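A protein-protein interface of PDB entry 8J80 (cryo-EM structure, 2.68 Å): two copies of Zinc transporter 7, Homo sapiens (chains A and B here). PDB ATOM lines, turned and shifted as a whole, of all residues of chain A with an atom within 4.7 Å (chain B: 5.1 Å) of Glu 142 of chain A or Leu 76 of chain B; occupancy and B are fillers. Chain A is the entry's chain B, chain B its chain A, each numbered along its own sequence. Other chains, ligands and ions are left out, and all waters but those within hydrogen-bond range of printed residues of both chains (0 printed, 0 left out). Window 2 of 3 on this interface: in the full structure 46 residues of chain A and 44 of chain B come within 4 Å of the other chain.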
ATOM      1  N   SER A 138      -5.252  25.764  20.252  1.00  0.00           N
ATOM      2  CA  SER A 138      -5.220  25.637  18.801  1.00  0.00           C
ATOM      3  C   SER A 138      -5.714  26.916  18.141  1.00  0.00           C
ATOM      4  O   SER A 138      -4.944  27.625  17.481  1.00  0.00           O
ATOM      5  CB  SER A 138      -6.059  24.438  18.362  1.00  0.00           C
ATOM      6  OG  SER A 138      -6.097  24.337  16.951  1.00  0.00           O
ATOM      7  N   GLU A 139      -6.976  27.277  18.395  1.00  0.00           N
ATOM      8  CA  GLU A 139      -7.510  28.494  17.799  1.00  0.00           C
ATOM      9  C   GLU A 139      -6.683  29.698  18.215  1.00  0.00           C
ATOM     10  O   GLU A 139      -6.434  30.599  17.405  1.00  0.00           O
ATOM     11  CB  GLU A 139      -8.977  28.678  18.188  1.00  0.00           C
ATOM     12  CG  GLU A 139      -9.515  30.091  17.993  1.00  0.00           C
ATOM     13  CD  GLU A 139      -9.670  30.494  16.532  1.00  0.00           C
ATOM     14  OE1 GLU A 139      -9.475  29.643  15.637  1.00  0.00           O
ATOM     15  OE2 GLU A 139      -9.978  31.677  16.276  1.00  0.00           O
ATOM     16  N   GLY A 140      -6.178  29.683  19.453  1.00  0.00           N
ATOM     17  CA  GLY A 140      -5.358  30.787  19.917  1.00  0.00           C
ATOM     18  C   GLY A 140      -4.129  30.980  19.057  1.00  0.00           C
ATOM     19  O   GLY A 140      -3.854  32.086  18.583  1.00  0.00           O
ATOM     20  N   VAL A 141      -3.414  29.888  18.775  1.00  0.00           N
ATOM     21  CA  VAL A 141      -2.204  30.054  17.989  1.00  0.00           C
ATOM     22  C   VAL A 141      -2.562  30.367  16.545  1.00  0.00           C
ATOM     23  O   VAL A 141      -1.736  30.933  15.817  1.00  0.00           O
ATOM     24  CB  VAL A 141      -1.284  28.825  18.132  1.00  0.00           C
ATOM     25  CG1 VAL A 141      -1.835  27.647  17.391  1.00  0.00           C
ATOM     26  CG2 VAL A 141       0.131  29.150  17.668  1.00  0.00           C
ATOM     27  N   GLU A 142      -3.801  30.072  16.131  1.00  0.00           N
ATOM     28  CA  GLU A 142      -4.288  30.573  14.851  1.00  0.00           C
ATOM     29  C   GLU A 142      -4.160  32.082  14.788  1.00  0.00           C
ATOM     30  O   GLU A 142      -3.560  32.636  13.859  1.00  0.00           O
ATOM     31  CB  GLU A 142      -5.748  30.171  14.627  1.00  0.00           C
ATOM     32  CG  GLU A 142      -6.122  29.808  13.182  1.00  0.00           C
ATOM     33  CD  GLU A 142      -5.300  28.689  12.550  1.00  0.00           C
ATOM     34  OE1 GLU A 142      -4.316  28.205  13.140  1.00  0.00           O
ATOM     35  OE2 GLU A 142      -5.617  28.325  11.402  1.00  0.00           O
ATOM     36  N   ARG A 143      -4.674  32.761  15.807  1.00  0.00           N
ATOM     37  CA  ARG A 143      -4.590  34.207  15.838  1.00  0.00           C
ATOM     38  C   ARG A 143      -3.173  34.688  16.103  1.00  0.00           C
ATOM     39  O   ARG A 143      -2.914  35.890  16.000  1.00  0.00           O
ATOM     40  CB  ARG A 143      -5.574  34.728  16.878  1.00  0.00           C
ATOM     41  CG  ARG A 143      -7.010  34.475  16.455  1.00  0.00           C
ATOM     42  CD  ARG A 143      -7.860  34.003  17.613  1.00  0.00           C
ATOM     43  NE  ARG A 143      -9.266  34.341  17.437  1.00  0.00           N
ATOM     44  CZ  ARG A 143      -9.781  35.532  17.699  1.00  0.00           C
ATOM     45  NH1 ARG A 143      -9.033  36.524  18.151  1.00  0.00           N
ATOM     46  NH2 ARG A 143     -11.081  35.732  17.505  1.00  0.00           N
ATOM     47  N   ALA A 144      -2.254  33.780  16.440  1.00  0.00           N
ATOM     48  CA  ALA A 144      -0.843  34.142  16.445  1.00  0.00           C
ATOM     49  C   ALA A 144      -0.362  34.472  15.038  1.00  0.00           C
ATOM     50  O   ALA A 144       0.436  35.397  14.849  1.00  0.00           O
ATOM     51  CB  ALA A 144      -0.012  33.014  17.052  1.00  0.00           C
ATOM     52  N   LEU A 145      -0.840  33.729  14.037  1.00  0.00           N
ATOM     53  CA  LEU A 145      -0.382  33.958  12.670  1.00  0.00           C
ATOM     54  C   LEU A 145      -1.040  35.185  12.049  1.00  0.00           C
ATOM     55  O   LEU A 145      -0.355  36.023  11.452  1.00  0.00           O
ATOM     56  CB  LEU A 145      -0.648  32.719  11.814  1.00  0.00           C
ATOM     57  CG  LEU A 145      -0.029  31.406  12.299  1.00  0.00           C
ATOM     58  CD1 LEU A 145      -0.048  30.367  11.190  1.00  0.00           C
ATOM     59  CD2 LEU A 145       1.392  31.623  12.801  1.00  0.00           C
ATOM     60  N   ALA A 146      -2.360  35.312  12.180  1.00  0.00           N
ATOM     61  CA  ALA A 146      -3.114  36.425  11.608  1.00  0.00           C
ATOM     62  C   ALA A 146      -3.983  37.029  12.701  1.00  0.00           C
ATOM     63  O   ALA A 146      -5.151  36.650  12.863  1.00  0.00           O
ATOM     64  CB  ALA A 146      -3.957  35.970  10.419  1.00  0.00           C
ATOM     65  N   ASN B  74      -0.533  29.859   2.637  1.00  0.00           N
ATOM     66  CA  ASN B  74      -1.936  29.460   2.634  1.00  0.00           C
ATOM     67  C   ASN B  74      -2.409  29.132   4.047  1.00  0.00           C
ATOM     68  O   ASN B  74      -3.126  28.153   4.259  1.00  0.00           O
ATOM     69  CB  ASN B  74      -2.170  28.272   1.701  1.00  0.00           C
ATOM     70  CG  ASN B  74      -1.506  28.449   0.352  1.00  0.00           C
ATOM     71  OD1 ASN B  74      -0.281  28.467   0.248  1.00  0.00           O
ATOM     72  ND2 ASN B  74      -2.315  28.582  -0.693  1.00  0.00           N
ATOM     73  N   CYS B  75      -2.017  29.960   5.018  1.00  0.00           N
ATOM     74  CA  CYS B  75      -2.132  29.594   6.427  1.00  0.00           C
ATOM     75  C   CYS B  75      -3.585  29.480   6.877  1.00  0.00           C
ATOM     76  O   CYS B  75      -3.934  28.575   7.646  1.00  0.00           O
ATOM     77  CB  CYS B  75      -1.384  30.614   7.286  1.00  0.00           C
ATOM     78  SG  CYS B  75       0.214  31.124   6.609  1.00  0.00           S
ATOM     79  N   LEU B  76      -4.449  30.371   6.378  1.00  0.00           N
ATOM     80  CA  LEU B  76      -5.755  30.680   6.961  1.00  0.00           C
ATOM     81  C   LEU B  76      -6.628  29.463   7.260  1.00  0.00           C
ATOM     82  O   LEU B  76      -7.299  29.424   8.296  1.00  0.00           O
ATOM     83  CB  LEU B  76      -6.520  31.651   6.048  1.00  0.00           C
ATOM     84  CG  LEU B  76      -7.043  31.234   4.667  1.00  0.00           C
ATOM     85  CD1 LEU B  76      -8.167  32.165   4.237  1.00  0.00           C
ATOM     86  CD2 LEU B  76      -5.940  31.225   3.618  1.00  0.00           C
ATOM     87  N   GLY B  77      -6.637  28.471   6.375  1.00  0.00           N
ATOM     88  CA  GLY B  77      -7.398  27.265   6.637  1.00  0.00           C
ATOM     89  C   GLY B  77      -6.514  26.049   6.819  1.00  0.00           C
ATOM     90  O   GLY B  77      -6.826  25.139   7.601  1.00  0.00           O
ATOM     91  N   LEU B  78      -5.391  26.042   6.094  1.00  0.00           N
ATOM     92  CA  LEU B  78      -4.489  24.899   6.125  1.00  0.00           C
ATOM     93  C   LEU B  78      -3.930  24.669   7.521  1.00  0.00           C
ATOM     94  O   LEU B  78      -3.860  23.525   7.980  1.00  0.00           O
ATOM     95  CB  LEU B  78      -3.345  25.095   5.131  1.00  0.00           C
ATOM     96  CG  LEU B  78      -3.627  24.995   3.631  1.00  0.00           C
ATOM     97  CD1 LEU B  78      -2.357  24.612   2.888  1.00  0.00           C
ATOM     98  CD2 LEU B  78      -4.738  24.001   3.344  1.00  0.00           C
ATOM     99  N   ILE B  79      -3.516  25.736   8.207  1.00  0.00           N
ATOM    100  CA  ILE B  79      -2.847  25.555   9.492  1.00  0.00           C
ATOM    101  C   ILE B  79      -3.838  25.054  10.543  1.00  0.00           C
ATOM    102  O   ILE B  79      -3.500  24.206  11.383  1.00  0.00           O
ATOM    103  CB  ILE B  79      -2.133  26.858   9.906  1.00  0.00           C
ATOM    104  CG1 ILE B  79      -0.653  26.819   9.510  1.00  0.00           C
ATOM    105  CG2 ILE B  79      -2.143  27.031  11.390  1.00  0.00           C
ATOM    106  CD1 ILE B  79      -0.384  26.514   8.057  1.00  0.00           C
ATOM    107  N   SER B  80      -5.085  25.536  10.495  1.00  0.00           N
ATOM    108  CA  SER B  80      -6.119  24.996  11.379  1.00  0.00           C
ATOM    109  C   SER B  80      -6.391  23.527  11.080  1.00  0.00           C
ATOM    110  O   SER B  80      -6.576  22.721  12.003  1.00  0.00           O
ATOM    111  CB  SER B  80      -7.410  25.802  11.249  1.00  0.00           C
ATOM    112  OG  SER B  80      -8.407  25.299  12.121  1.00  0.00           O
ATOM    113  N   PHE B  83      -3.657  21.556  12.629  1.00  0.00           N
ATOM    114  CA  PHE B  83      -3.685  21.434  14.080  1.00  0.00           C
ATOM    115  C   PHE B  83      -4.798  20.496  14.530  1.00  0.00           C
ATOM    116  O   PHE B  83      -4.616  19.733  15.488  1.00  0.00           O
ATOM    117  CB  PHE B  83      -3.794  22.826  14.701  1.00  0.00           C
ATOM    118  CG  PHE B  83      -2.546  23.656  14.513  1.00  0.00           C
ATOM    119  CD1 PHE B  83      -1.392  23.086  13.989  1.00  0.00           C
ATOM    120  CD2 PHE B  83      -2.535  25.004  14.813  1.00  0.00           C
ATOM    121  CE1 PHE B  83      -0.250  23.835  13.796  1.00  0.00           C
ATOM    122  CE2 PHE B  83      -1.389  25.758  14.614  1.00  0.00           C
ATOM    123  CZ  PHE B  83      -0.249  25.171  14.110  1.00  0.00           C
ATOM    124  N   HIS B 152     -10.776  29.165   1.736  1.00  0.00           N
ATOM    125  CA  HIS B 152      -9.586  28.979   0.918  1.00  0.00           C
ATOM    126  C   HIS B 152      -9.072  27.550   1.121  1.00  0.00           C
ATOM    127  O   HIS B 152      -7.903  27.320   1.429  1.00  0.00           O
ATOM    128  CB  HIS B 152      -8.505  30.017   1.234  1.00  0.00           C
ATOM    129  CG  HIS B 152      -7.391  30.046   0.235  1.00  0.00           C
ATOM    130  ND1 HIS B 152      -6.076  29.801   0.573  1.00  0.00           N
ATOM    131  CD2 HIS B 152      -7.398  30.283  -1.099  1.00  0.00           C
ATOM    132  CE1 HIS B 152      -5.322  29.886  -0.509  1.00  0.00           C
ATOM    133  NE2 HIS B 152      -6.099  30.179  -1.537  1.00  0.00           N
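The side-chain carboxylate (OE2) of Glu 142 of chain A is in hydrogen-bond range of the backbone NH (N) of Ser 80 of chain B, 3.0 Å away.
No position is printed for both chains. Of the 6 pairs that touch across the chains among the printed residues, none has its exchanged pair printed and touching as well.
Along chain B the printed residues that touch a printed residue of chain A span positions 76 to 83. Hydrophobic or aromatic side chains of chain A within 4 Å of the printed part of chain B: Val 141 and Leu 145. Among the printed residues, no Asp or Glu carboxylate lies within 4 Å of a Lys or Arg side-chain nitrogen of the other chain.
Of chain B, only Leu 76 (3.7 Å), Ile 79 (3.0 Å) and Ser 80 (3.0 Å) come within 4 Å of Glu 142 of chain A. Leu 76 of chain B touches one residue of chain A. Of the printed residues of chain B, Ser 138 of chain A touches Phe 83. Printed residues of chain B within 4 Å of Val 141 of chain A: Phe 83. Of the printed residues of chain A, Ser 80 of chain B touches Glu 142 (3.0 Å). The nearest residue of chain B that does not touch Glu 142 of chain A is Phe 83 of chain B (4.03 Å). The nearest printed residue of chain A that does not touch Ile 79 of chain B is Val 141 of chain A (5.9 Å).
Ser 138 of chain A touches Phe 83 of chain B (OG to CB, 3.6 Å). Phe 83 of chain B touches Val 141 of chain A. Glu 142 of chain A touches Leu 76 of chain B. Ile 79 of chain B touches Glu 142 of chain A (CG2 to OE1, 3.0 Å). CG2 of Ile 79 of chain B touches CD1 of Leu 145 of chain A, at 3.9 Å.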
